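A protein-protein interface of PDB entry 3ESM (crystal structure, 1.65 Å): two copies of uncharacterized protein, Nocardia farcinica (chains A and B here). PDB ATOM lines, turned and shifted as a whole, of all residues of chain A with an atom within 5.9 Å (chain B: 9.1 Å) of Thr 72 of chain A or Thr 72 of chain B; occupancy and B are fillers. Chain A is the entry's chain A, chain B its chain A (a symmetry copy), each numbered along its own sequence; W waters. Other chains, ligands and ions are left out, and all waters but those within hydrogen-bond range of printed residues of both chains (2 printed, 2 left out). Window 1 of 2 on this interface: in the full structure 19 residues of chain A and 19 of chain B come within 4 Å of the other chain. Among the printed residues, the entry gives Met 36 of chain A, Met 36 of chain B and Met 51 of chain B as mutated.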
ATOM      1  N   THR A  34       4.452  32.237  14.450  1.00  0.00           N
ATOM      2  CA  THR A  34       4.895  30.963  15.076  1.00  0.00           C
ATOM      3  C   THR A  34       3.849  29.861  15.140  1.00  0.00           C
ATOM      4  O   THR A  34       4.183  28.690  15.388  1.00  0.00           O
ATOM      5  CB  THR A  34       5.427  31.187  16.493  1.00  0.00           C
ATOM      6  OG1 THR A  34       4.385  31.756  17.309  1.00  0.00           O
ATOM      7  CG2 THR A  34       6.651  32.122  16.429  1.00  0.00           C
ATOM      8  N   ALA A  35       2.597  30.198  14.855  1.00  0.00           N
ATOM      9  CA  ALA A  35       1.572  29.139  14.732  1.00  0.00           C
ATOM     10  C   ALA A  35       0.409  29.667  13.911  1.00  0.00           C
ATOM     11  O   ALA A  35       0.177  30.884  13.826  1.00  0.00           O
ATOM     12  CB  ALA A  35       1.075  28.726  16.086  1.00  0.00           C
ATOM     13  N   MET A  36      -0.313  28.739  13.325  1.00  0.00           N
ATOM     14  CA  MET A  36      -1.523  29.088  12.580  1.00  0.00           C
ATOM     15  C   MET A  36      -2.564  28.036  12.878  1.00  0.00           C
ATOM     16  O   MET A  36      -2.285  26.847  12.704  1.00  0.00           O
ATOM     17  CB  MET A  36      -1.202  29.087  11.082  1.00  0.00           C
ATOM     18  CG  MET A  36      -2.391  29.318  10.166  1.00  0.00           C
ATOM     19  SD  MET A  36      -2.965  31.058  10.185  1.00  0.00           S
ATOM     20  CE  MET A  36      -1.467  31.853  10.521  1.00  0.00           C
ATOM     21  N   GLY A  53      10.395  21.679  10.264  1.00  0.00           N
ATOM     22  CA  GLY A  53      10.436  22.718  11.283  1.00  0.00           C
ATOM     23  C   GLY A  53       9.088  23.067  11.869  1.00  0.00           C
ATOM     24  O   GLY A  53       9.019  23.924  12.745  1.00  0.00           O
ATOM     25  N   TRP A  54       8.020  22.429  11.393  1.00  0.00           N
ATOM     26  CA  TRP A  54       6.660  22.697  11.940  1.00  0.00           C
ATOM     27  C   TRP A  54       5.988  21.384  12.296  1.00  0.00           C
ATOM     28  O   TRP A  54       6.247  20.342  11.641  1.00  0.00           O
ATOM     29  CB  TRP A  54       5.788  23.383  10.882  1.00  0.00           C
ATOM     30  CG  TRP A  54       6.303  24.729  10.477  1.00  0.00           C
ATOM     31  CD1 TRP A  54       7.383  25.002   9.651  1.00  0.00           C
ATOM     32  CD2 TRP A  54       5.790  25.993  10.894  1.00  0.00           C
ATOM     33  NE1 TRP A  54       7.541  26.379   9.523  1.00  0.00           N
ATOM     34  CE2 TRP A  54       6.570  27.006  10.254  1.00  0.00           C
ATOM     35  CE3 TRP A  54       4.714  26.371  11.681  1.00  0.00           C
ATOM     36  CZ2 TRP A  54       6.353  28.381  10.474  1.00  0.00           C
ATOM     37  CZ3 TRP A  54       4.473  27.777  11.873  1.00  0.00           C
ATOM     38  CH2 TRP A  54       5.290  28.745  11.260  1.00  0.00           C
ATOM     39  N   THR A  55       5.151  21.403  13.325  1.00  0.00           N
ATOM     40  CA  THR A  55       4.355  20.242  13.658  1.00  0.00           C
ATOM     41  C   THR A  55       2.899  20.564  13.398  1.00  0.00           C
ATOM     42  O   THR A  55       2.463  21.653  13.697  1.00  0.00           O
ATOM     43  CB  THR A  55       4.569  19.830  15.119  1.00  0.00           C
ATOM     44  OG1 THR A  55       5.950  19.383  15.243  1.00  0.00           O
ATOM     45  CG2 THR A  55       3.619  18.693  15.472  1.00  0.00           C
ATOM     46  N   ALA A  56       2.160  19.637  12.796  1.00  0.00           N
ATOM     47  CA  ALA A  56       0.736  19.869  12.536  1.00  0.00           C
ATOM     48  C   ALA A  56      -0.135  18.894  13.336  1.00  0.00           C
ATOM     49  O   ALA A  56       0.230  17.700  13.519  1.00  0.00           O
ATOM     50  CB  ALA A  56       0.423  19.769  11.057  1.00  0.00           C
ATOM     51  N   ARG A  57      -1.265  19.400  13.832  1.00  0.00           N
ATOM     52  CA  ARG A  57      -2.274  18.542  14.457  1.00  0.00           C
ATOM     53  C   ARG A  57      -3.595  18.838  13.758  1.00  0.00           C
ATOM     54  O   ARG A  57      -3.885  19.992  13.435  1.00  0.00           O
ATOM     55  CB  ARG A  57      -2.462  18.768  15.970  1.00  0.00           C
ATOM     56  CG  ARG A  57      -2.928  20.120  16.386  1.00  0.00           C
ATOM     57  CD  ARG A  57      -3.009  20.189  17.941  1.00  0.00           C
ATOM     58  NE  ARG A  57      -4.172  19.482  18.480  1.00  0.00           N
ATOM     59  CZ  ARG A  57      -4.137  18.454  19.331  1.00  0.00           C
ATOM     60  NH1 ARG A  57      -2.976  17.953  19.789  1.00  0.00           N
ATOM     61  NH2 ARG A  57      -5.287  17.932  19.731  1.00  0.00           N
ATOM     62  N   THR A  70      -3.868  22.791  13.117  1.00  0.00           N
ATOM     63  CA  THR A  70      -2.952  23.790  13.679  1.00  0.00           C
ATOM     64  C   THR A  70      -1.537  23.435  13.294  1.00  0.00           C
ATOM     65  O   THR A  70      -1.136  22.256  13.418  1.00  0.00           O
ATOM     66  CB  THR A  70      -3.010  23.843  15.213  1.00  0.00           C
ATOM     67  OG1 THR A  70      -4.314  24.205  15.661  1.00  0.00           O
ATOM     68  CG2 THR A  70      -1.964  24.848  15.758  1.00  0.00           C
ATOM     69  N   TRP A  71      -0.788  24.403  12.774  1.00  0.00           N
ATOM     70  CA  TRP A  71       0.659  24.210  12.520  1.00  0.00           C
ATOM     71  C   TRP A  71       1.414  25.046  13.533  1.00  0.00           C
ATOM     72  O   TRP A  71       1.034  26.196  13.794  1.00  0.00           O
ATOM     73  CB  TRP A  71       1.026  24.726  11.130  1.00  0.00           C
ATOM     74  CG  TRP A  71       0.471  23.964  10.000  1.00  0.00           C
ATOM     75  CD1 TRP A  71       1.089  22.935   9.336  1.00  0.00           C
ATOM     76  CD2 TRP A  71      -0.778  24.194   9.330  1.00  0.00           C
ATOM     77  NE1 TRP A  71       0.284  22.501   8.303  1.00  0.00           N
ATOM     78  CE2 TRP A  71      -0.867  23.249   8.277  1.00  0.00           C
ATOM     79  CE3 TRP A  71      -1.835  25.095   9.535  1.00  0.00           C
ATOM     80  CZ2 TRP A  71      -1.948  23.211   7.384  1.00  0.00           C
ATOM     81  CZ3 TRP A  71      -2.922  25.055   8.664  1.00  0.00           C
ATOM     82  CH2 TRP A  71      -2.982  24.106   7.611  1.00  0.00           C
ATOM     83  N   THR A  72       2.492  24.503  14.091  1.00  0.00           N
ATOM     84  CA  THR A  72       3.221  25.187  15.158  1.00  0.00           C
ATOM     85  C   THR A  72       4.685  25.060  14.855  1.00  0.00           C
ATOM     86  O   THR A  72       5.155  23.957  14.560  1.00  0.00           O
ATOM     87  CB  THR A  72       2.982  24.524  16.519  1.00  0.00           C
ATOM     88  OG1 THR A  72       1.570  24.497  16.792  1.00  0.00           O
ATOM     89  CG2 THR A  72       3.704  25.340  17.621  1.00  0.00           C
ATOM     90  N   ALA A  73       5.404  26.182  14.936  1.00  0.00           N
ATOM     91  CA  ALA A  73       6.850  26.168  14.661  1.00  0.00           C
ATOM     92  C   ALA A  73       7.581  25.432  15.785  1.00  0.00           C
ATOM     93  O   ALA A  73       7.332  25.692  16.969  1.00  0.00           O
ATOM     94  CB  ALA A  73       7.327  27.625  14.557  1.00  0.00           C
ATOM     95  N   ASP A  74       8.369  24.406  15.416  1.00  0.00           N
ATOM     96  CA  ASP A  74       9.214  23.718  16.389  1.00  0.00           C
ATOM     97  C   ASP A  74      10.168  24.654  17.120  1.00  0.00           C
ATOM     98  O   ASP A  74      10.615  25.642  16.590  1.00  0.00           O
ATOM     99  CB  ASP A  74      10.065  22.650  15.701  1.00  0.00           C
ATOM    100  CG  ASP A  74       9.230  21.608  15.008  1.00  0.00           C
ATOM    101  OD1 ASP A  74       8.048  21.475  15.353  1.00  0.00           O
ATOM    102  OD2 ASP A  74       9.773  20.947  14.091  1.00  0.00           O
ATOM    103  N   THR B  33      -8.797  22.427  25.303  1.00  0.00           N
ATOM    104  CA  THR B  33      -7.687  23.361  25.142  1.00  0.00           C
ATOM    105  C   THR B  33      -6.507  22.600  24.514  1.00  0.00           C
ATOM    106  O   THR B  33      -6.034  21.607  25.088  1.00  0.00           O
ATOM    107  CB  THR B  33      -7.219  23.934  26.474  1.00  0.00           C
ATOM    108  OG1 THR B  33      -8.295  24.688  27.047  1.00  0.00           O
ATOM    109  CG2 THR B  33      -5.998  24.851  26.249  1.00  0.00           C
ATOM    110  N   THR B  34      -6.013  23.131  23.398  1.00  0.00           N
ATOM    111  CA  THR B  34      -4.898  22.493  22.650  1.00  0.00           C
ATOM    112  C   THR B  34      -3.612  23.301  22.567  1.00  0.00           C
ATOM    113  O   THR B  34      -2.551  22.762  22.210  1.00  0.00           O
ATOM    114  CB  THR B  34      -5.313  22.126  21.224  1.00  0.00           C
ATOM    115  OG1 THR B  34      -5.709  23.319  20.520  1.00  0.00           O
ATOM    116  CG2 THR B  34      -6.471  21.111  21.282  1.00  0.00           C
ATOM    117  N   ALA B  35      -3.670  24.570  22.954  1.00  0.00           N
ATOM    118  CA  ALA B  35      -2.419  25.352  23.060  1.00  0.00           C
ATOM    119  C   ALA B  35      -2.647  26.530  23.990  1.00  0.00           C
ATOM    120  O   ALA B  35      -3.784  26.992  24.183  1.00  0.00           O
ATOM    121  CB  ALA B  35      -1.999  25.859  21.712  1.00  0.00           C
ATOM    122  N   MET B  36      -1.557  27.007  24.547  1.00  0.00           N
ATOM    123  CA  MET B  36      -1.605  28.201  25.391  1.00  0.00           C
ATOM    124  C   MET B  36      -0.385  29.033  25.079  1.00  0.00           C
ATOM    125  O   MET B  36       0.731  28.511  25.143  1.00  0.00           O
ATOM    126  CB  MET B  36      -1.576  27.773  26.861  1.00  0.00           C
ATOM    127  CG  MET B  36      -1.503  28.910  27.865  1.00  0.00           C
ATOM    128  SD  MET B  36      -3.087  29.817  28.015  1.00  0.00           S
ATOM    129  CE  MET B  36      -4.190  28.537  27.648  1.00  0.00           C
ATOM    130  N   THR B  37      -0.580  30.326  24.807  1.00  0.00           N
ATOM    131  CA  THR B  37       0.552  31.210  24.587  1.00  0.00           C
ATOM    132  C   THR B  37       0.516  32.274  25.672  1.00  0.00           C
ATOM    133  O   THR B  37      -0.523  32.872  25.865  1.00  0.00           O
ATOM    134  CB  THR B  37       0.478  31.860  23.180  1.00  0.00           C
ATOM    135  OG1 THR B  37       0.868  30.852  22.201  1.00  0.00           O
ATOM    136  CG2 THR B  37       1.457  33.008  23.075  1.00  0.00           C
ATOM    137  N   THR B  48      10.764  26.129  30.698  1.00  0.00           N
ATOM    138  CA  THR B  48       9.583  25.348  31.007  1.00  0.00           C
ATOM    139  C   THR B  48       9.970  24.009  31.600  1.00  0.00           C
ATOM    140  O   THR B  48      11.131  23.578  31.541  1.00  0.00           O
ATOM    141  CB  THR B  48       8.740  25.073  29.743  1.00  0.00           C
ATOM    142  OG1 THR B  48       9.561  24.448  28.742  1.00  0.00           O
ATOM    143  CG2 THR B  48       8.181  26.388  29.194  1.00  0.00           C
ATOM    144  N   MET B  51       6.528  18.376  30.034  1.00  0.00           N
ATOM    145  CA  MET B  51       5.094  18.165  30.144  1.00  0.00           C
ATOM    146  C   MET B  51       4.766  17.075  29.115  1.00  0.00           C
ATOM    147  O   MET B  51       4.632  17.402  27.931  1.00  0.00           O
ATOM    148  CB  MET B  51       4.429  19.507  29.755  1.00  0.00           C
ATOM    149  CG  MET B  51       2.942  19.654  29.968  1.00  0.00           C
ATOM    150  SD  MET B  51       2.380  21.398  29.752  1.00  0.00           S
ATOM    151  CE  MET B  51       0.633  21.147  29.921  1.00  0.00           C
ATOM    152  N   PRO B  52       4.655  15.796  29.533  1.00  0.00           N
ATOM    153  CA  PRO B  52       4.401  14.760  28.545  1.00  0.00           C
ATOM    154  C   PRO B  52       3.192  15.095  27.682  1.00  0.00           C
ATOM    155  O   PRO B  52       2.135  15.523  28.209  1.00  0.00           O
ATOM    156  CB  PRO B  52       4.155  13.500  29.404  1.00  0.00           C
ATOM    157  CG  PRO B  52       4.986  13.776  30.624  1.00  0.00           C
ATOM    158  CD  PRO B  52       4.714  15.245  30.903  1.00  0.00           C
ATOM    159  N   GLY B  53       3.357  14.909  26.383  1.00  0.00           N
ATOM    160  CA  GLY B  53       2.270  15.154  25.446  1.00  0.00           C
ATOM    161  C   GLY B  53       2.166  16.585  24.974  1.00  0.00           C
ATOM    162  O   GLY B  53       1.289  16.889  24.172  1.00  0.00           O
ATOM    163  N   TRP B  54       3.036  17.465  25.466  1.00  0.00           N
ATOM    164  CA  TRP B  54       3.016  18.889  25.027  1.00  0.00           C
ATOM    165  C   TRP B  54       4.414  19.313  24.613  1.00  0.00           C
ATOM    166  O   TRP B  54       5.421  18.803  25.170  1.00  0.00           O
ATOM    167  CB  TRP B  54       2.589  19.797  26.187  1.00  0.00           C
ATOM    168  CG  TRP B  54       1.195  19.529  26.661  1.00  0.00           C
ATOM    169  CD1 TRP B  54       0.761  18.464  27.436  1.00  0.00           C
ATOM    170  CD2 TRP B  54       0.038  20.313  26.375  1.00  0.00           C
ATOM    171  NE1 TRP B  54      -0.609  18.573  27.659  1.00  0.00           N
ATOM    172  CE2 TRP B  54      -1.070  19.702  27.040  1.00  0.00           C
ATOM    173  CE3 TRP B  54      -0.162  21.499  25.687  1.00  0.00           C
ATOM    174  CZ2 TRP B  54      -2.384  20.204  26.940  1.00  0.00           C
ATOM    175  CZ3 TRP B  54      -1.498  22.028  25.620  1.00  0.00           C
ATOM    176  CH2 TRP B  54      -2.572  21.375  26.252  1.00  0.00           C
ATOM    177  N   THR B  55       4.501  20.214  23.644  1.00  0.00           N
ATOM    178  CA  THR B  55       5.777  20.786  23.273  1.00  0.00           C
ATOM    179  C   THR B  55       5.774  22.253  23.648  1.00  0.00           C
ATOM    180  O   THR B  55       4.780  22.918  23.460  1.00  0.00           O
ATOM    181  CB  THR B  55       6.045  20.608  21.774  1.00  0.00           C
ATOM    182  OG1 THR B  55       6.193  19.179  21.530  1.00  0.00           O
ATOM    183  CG2 THR B  55       7.326  21.338  21.395  1.00  0.00           C
ATOM    184  N   ALA B  56       6.868  22.745  24.222  1.00  0.00           N
ATOM    185  CA  ALA B  56       6.946  24.163  24.587  1.00  0.00           C
ATOM    186  C   ALA B  56       8.026  24.882  23.770  1.00  0.00           C
ATOM    187  O   ALA B  56       9.107  24.302  23.474  1.00  0.00           O
ATOM    188  CB  ALA B  56       7.200  24.335  26.070  1.00  0.00           C
ATOM    189  N   ARG B  57       7.730  26.124  23.386  1.00  0.00           N
ATOM    190  CA  ARG B  57       8.734  26.988  22.761  1.00  0.00           C
ATOM    191  C   ARG B  57       8.757  28.285  23.562  1.00  0.00           C
ATOM    192  O   ARG B  57       7.709  28.772  23.991  1.00  0.00           O
ATOM    193  CB  ARG B  57       8.458  27.333  21.285  1.00  0.00           C
ATOM    194  CG  ARG B  57       7.205  28.088  21.004  1.00  0.00           C
ATOM    195  CD  ARG B  57       7.057  28.300  19.467  1.00  0.00           C
ATOM    196  NE  ARG B  57       7.950  29.337  18.949  1.00  0.00           N
ATOM    197  CZ  ARG B  57       8.895  29.164  18.021  1.00  0.00           C
ATOM    198  NH1 ARG B  57       9.120  27.966  17.454  1.00  0.00           N
ATOM    199  NH2 ARG B  57       9.613  30.216  17.655  1.00  0.00           N
ATOM    200  N   ASP B  59       9.937  32.110  22.934  1.00  0.00           N
ATOM    201  CA  ASP B  59      10.405  33.035  21.890  1.00  0.00           C
ATOM    202  C   ASP B  59      11.249  34.166  22.493  1.00  0.00           C
ATOM    203  O   ASP B  59      11.005  34.591  23.615  1.00  0.00           O
ATOM    204  CB  ASP B  59       9.243  33.621  21.114  1.00  0.00           C
ATOM    205  CG  ASP B  59       8.723  32.634  20.052  1.00  0.00           C
ATOM    206  OD1 ASP B  59       9.257  32.663  18.913  1.00  0.00           O
ATOM    207  OD2 ASP B  59       7.845  31.821  20.381  1.00  0.00           O
ATOM    208  N   VAL B  69       5.899  32.456  25.707  1.00  0.00           N
ATOM    209  CA  VAL B  69       6.119  30.999  25.797  1.00  0.00           C
ATOM    210  C   VAL B  69       4.850  30.376  25.279  1.00  0.00           C
ATOM    211  O   VAL B  69       3.741  30.892  25.530  1.00  0.00           O
ATOM    212  CB  VAL B  69       6.420  30.536  27.239  1.00  0.00           C
ATOM    213  CG1 VAL B  69       5.394  31.095  28.257  1.00  0.00           C
ATOM    214  CG2 VAL B  69       6.492  28.994  27.317  1.00  0.00           C
ATOM    215  N   THR B  70       4.991  29.285  24.521  1.00  0.00           N
ATOM    216  CA  THR B  70       3.793  28.632  23.981  1.00  0.00           C
ATOM    217  C   THR B  70       3.877  27.149  24.248  1.00  0.00           C
ATOM    218  O   THR B  70       4.939  26.532  24.009  1.00  0.00           O
ATOM    219  CB  THR B  70       3.657  28.816  22.461  1.00  0.00           C
ATOM    220  OG1 THR B  70       3.540  30.197  22.126  1.00  0.00           O
ATOM    221  CG2 THR B  70       2.429  28.035  21.932  1.00  0.00           C
ATOM    222  N   TRP B  71       2.811  26.569  24.793  1.00  0.00           N
ATOM    223  CA  TRP B  71       2.721  25.097  24.941  1.00  0.00           C
ATOM    224  C   TRP B  71       1.688  24.604  23.949  1.00  0.00           C
ATOM    225  O   TRP B  71       0.625  25.222  23.801  1.00  0.00           O
ATOM    226  CB  TRP B  71       2.230  24.734  26.341  1.00  0.00           C
ATOM    227  CG  TRP B  71       3.158  25.039  27.441  1.00  0.00           C
ATOM    228  CD1 TRP B  71       4.079  24.181  27.985  1.00  0.00           C
ATOM    229  CD2 TRP B  71       3.229  26.254  28.203  1.00  0.00           C
ATOM    230  NE1 TRP B  71       4.731  24.802  29.029  1.00  0.00           N
ATOM    231  CE2 TRP B  71       4.236  26.073  29.184  1.00  0.00           C
ATOM    232  CE3 TRP B  71       2.550  27.482  28.134  1.00  0.00           C
ATOM    233  CZ2 TRP B  71       4.548  27.053  30.137  1.00  0.00           C
ATOM    234  CZ3 TRP B  71       2.864  28.469  29.066  1.00  0.00           C
ATOM    235  CH2 TRP B  71       3.870  28.258  30.045  1.00  0.00           C
ATOM    236  N   THR B  72       1.964  23.485  23.286  1.00  0.00           N
ATOM    237  CA  THR B  72       1.082  22.989  22.230  1.00  0.00           C
ATOM    238  C   THR B  72       0.927  21.511  22.430  1.00  0.00           C
ATOM    239  O   THR B  72       1.928  20.810  22.610  1.00  0.00           O
ATOM    240  CB  THR B  72       1.693  23.197  20.840  1.00  0.00           C
ATOM    241  OG1 THR B  72       1.990  24.591  20.654  1.00  0.00           O
ATOM    242  CG2 THR B  72       0.680  22.737  19.761  1.00  0.00           C
ATOM    243  N   ALA B  73      -0.320  21.036  22.392  1.00  0.00           N
ATOM    244  CA  ALA B  73      -0.583  19.601  22.573  1.00  0.00           C
ATOM    245  C   ALA B  73      -0.083  18.826  21.353  1.00  0.00           C
ATOM    246  O   ALA B  73      -0.360  19.212  20.210  1.00  0.00           O
ATOM    247  CB  ALA B  73      -2.097  19.415  22.758  1.00  0.00           C
ATOM    248  N   ASP B  74       0.783  17.824  21.592  1.00  0.00           N
ATOM    249  CA  ASP B  74       1.223  16.937  20.518  1.00  0.00           C
ATOM    250  C   ASP B  74       0.069  16.246  19.803  1.00  0.00           C
ATOM    251  O   ASP B  74      -0.955  15.966  20.378  1.00  0.00           O
ATOM    252  CB  ASP B  74       2.136  15.841  21.068  1.00  0.00           C
ATOM    253  CG  ASP B  74       3.367  16.397  21.730  1.00  0.00           C
ATOM    254  OD1 ASP B  74       3.715  17.552  21.451  1.00  0.00           O
ATOM    255  OD2 ASP B  74       3.960  15.665  22.557  1.00  0.00           O
ATOM    256  N   PRO B  75       0.293  15.886  18.539  1.00  0.00           N
ATOM    257  CA  PRO B  75      -0.702  15.118  17.760  1.00  0.00           C
ATOM    258  C   PRO B  75      -1.091  13.840  18.519  1.00  0.00           C
ATOM    259  O   PRO B  75      -0.212  13.129  19.046  1.00  0.00           O
ATOM    260  CB  PRO B  75       0.071  14.801  16.473  1.00  0.00           C
ATOM    261  CG  PRO B  75       0.974  15.964  16.316  1.00  0.00           C
ATOM    262  CD  PRO B  75       1.456  16.253  17.742  1.00  0.00           C
ATOM    263  N   ASN B  77      -2.643  13.740  21.347  1.00  0.00           N
ATOM    264  CA  ASN B  77      -3.077  14.232  22.646  1.00  0.00           C
ATOM    265  C   ASN B  77      -4.327  15.063  22.432  1.00  0.00           C
ATOM    266  O   ASN B  77      -4.252  16.067  21.717  1.00  0.00           O
ATOM    267  CB  ASN B  77      -1.943  15.080  23.238  1.00  0.00           C
ATOM    268  CG  ASN B  77      -2.281  15.642  24.598  1.00  0.00           C
ATOM    269  OD1 ASN B  77      -3.406  15.490  25.085  1.00  0.00           O
ATOM    270  ND2 ASN B  77      -1.309  16.304  25.227  1.00  0.00           N
ATOM    271  N   GLY B  79      -5.797  17.098  24.244  1.00  0.00           N
ATOM    272  CA  GLY B  79      -5.798  18.378  24.970  1.00  0.00           C
ATOM    273  C   GLY B  79      -6.666  18.367  26.221  1.00  0.00           C
ATOM    274  O   GLY B  79      -7.139  17.304  26.656  1.00  0.00           O
ATOM    275  N   PHE B  88       0.346  24.986  33.486  1.00  0.00           N
ATOM    276  CA  PHE B  88       1.434  25.206  32.545  1.00  0.00           C
ATOM    277  C   PHE B  88       2.456  25.975  33.370  1.00  0.00           C
ATOM    278  O   PHE B  88       2.140  27.053  33.911  1.00  0.00           O
ATOM    279  CB  PHE B  88       0.938  26.069  31.389  1.00  0.00           C
ATOM    280  CG  PHE B  88      -0.085  25.396  30.528  1.00  0.00           C
ATOM    281  CD1 PHE B  88       0.308  24.624  29.442  1.00  0.00           C
ATOM    282  CD2 PHE B  88      -1.442  25.541  30.803  1.00  0.00           C
ATOM    283  CE1 PHE B  88      -0.638  23.999  28.641  1.00  0.00           C
ATOM    284  CE2 PHE B  88      -2.389  24.915  30.000  1.00  0.00           C
ATOM    285  CZ  PHE B  88      -1.977  24.149  28.932  1.00  0.00           C
ATOM    286  N   THR B 108      -5.981  28.393  22.886  1.00  0.00           N
ATOM    287  CA  THR B 108      -6.551  27.835  21.685  1.00  0.00           C
ATOM    288  C   THR B 108      -7.368  26.603  22.016  1.00  0.00           C
ATOM    289  O   THR B 108      -6.894  25.741  22.793  1.00  0.00           O
ATOM    290  CB  THR B 108      -5.425  27.404  20.699  1.00  0.00           C
ATOM    291  OG1 THR B 108      -4.662  28.554  20.268  1.00  0.00           O
ATOM    292  CG2 THR B 108      -6.020  26.706  19.498  1.00  0.00           C
HETATM  293  O   HOH W   1       3.126  29.798  19.137  1.00  0.00           O
HETATM  294  O   HOH W   2      -3.653  24.302  18.629  1.00  0.00           O
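The backbone carbonyl oxygen of Ala 73 of chain B sits at hydrogen-bond distance from the guanidinium group of Arg 57 of chain A (2.9 Å). The guanidinium group of Arg 57 of chain A sits at hydrogen-bond distance from the backbone carbonyl oxygen of Asp 74 of chain B, 2.9 Å away. The guanidinium group of Arg 57 of chain A is in hydrogen-bond range of the backbone carbonyl oxygen of Asn 77 of chain B. The backbone carbonyl oxygen of Ala 73 of chain A lies within hydrogen-bond range of the guanidinium group of Arg 57 of chain B (2.9 Å). The backbone carbonyl oxygen (O) of Asp 74 of chain A is in hydrogen-bond range of the guanidinium group (NH1) of Arg 57 of chain B, at 2.9 Å.
The backbone carbonyl oxygen of Gly 53 of chain A is in hydrogen-bond range of the backbone NH of Asp 74 of chain A (2.8 Å). The backbone NH of Thr 70 of chain A sits at hydrogen-bond distance from the backbone carbonyl oxygen of Arg 57 of chain A (2.8 Å). The backbone carbonyl oxygen (O) of Thr 34 of chain B sits at hydrogen-bond distance from the backbone NH (N) of Ala 73 of chain B, 2.8 Å away. ND2 of Asn 77 of chain B lies close to NE1 of Trp 54 of chain B (3.4 Å). N of Thr 55 of chain B is in hydrogen-bond range of O of Thr 72 of chain B, at 2.8 Å. OD1 of Asp 74 of chain B sits at hydrogen-bond distance from OG1 of Thr 55 of chain B (3.0 Å).
Arg 57 of chain B touches Thr 34 of chain A (NH2 to CG2, 3.7 Å). Asp 59 of chain B touches Thr 34 of chain A (OD1 to CG2, 3.6 Å). Pro 75 of chain B touches Thr 55 of chain A. Ala 56 of chain A touches Pro 75 of chain B (O to CG, 3.4 Å). Thr 34 of chain B touches Arg 57 of chain A. OG1 of Thr 72 of chain B touches CG2 of Thr 72 of chain A, at 3.6 Å.
Thr 72 of chain A touches one residue of chain B. Thr 72 of chain B touches just one residue of chain A: Thr 72. Of the printed residues of chain B, Asp 74 of chain A touches Arg 57 (2.9 Å). Printed residues of chain A within 4 Å of Ala 73 of chain B: Arg 57. Of the printed residues of chain A, Asp 74 of chain B touches Arg 57 (2.9 Å). Of the printed residues of chain A, Asn 77 of chain B touches Arg 57 (2.9 Å). Printed residues of chain B within 4 Å of Arg 57 of chain A: Thr 34, Ala 73, Asp 74 and Asn 77. Gly 53 of chain A touches none of the printed residues of chain B. The nearest residue of chain B that does not touch Thr 72 of chain A is Arg 57 of chain B (4.8 Å). The nearest residue of chain A that does not touch Thr 72 of chain B is Arg 57 of chain A (4.8 Å).
Of the 25 printed residues of chain B, 8 touch a printed residue of chain A. Printed residues of chain B that touch a printed residue of chain A: Thr 34, Arg 57, Asp 59, Thr 72, Ala 73, Asp 74, Pro 75 and Asn 77. Of the 13 printed residues of chain A, 7 touch a printed residue of chain B. Hydrophobic or aromatic side chains of chain A that line the printed part of chain B: Ala 73.
Thr 34 of chain A touches Arg 57 of chain B, and with the chains exchanged Arg 57 of chain A touches Thr 34 of chain B. Arg 57 of chain A touches Ala 73 of chain B, and with the chains exchanged Ala 73 of chain A touches Arg 57 of chain B. Arg 57 of chain A touches Asp 74 of chain B, and with the chains exchanged Asp 74 of chain A touches Arg 57 of chain B. Thr 72 of chain A touches its own counterpart, Thr 72 of chain B. Of the 11 pairs that touch across the chains among the printed residues, 7 have their exchanged pair printed and touching as well.
Water W1 bridges OG1 of Thr 34 of chain A (3.0 Å) and OG1 of Thr 70 of chain B (3.0 Å). Water W2 lies within hydrogen-bond range of the side-chain hydroxyl of Thr 34 of chain B (3.0 Å) and the side-chain hydroxyl of Thr 70 of chain A (3.0 Å).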
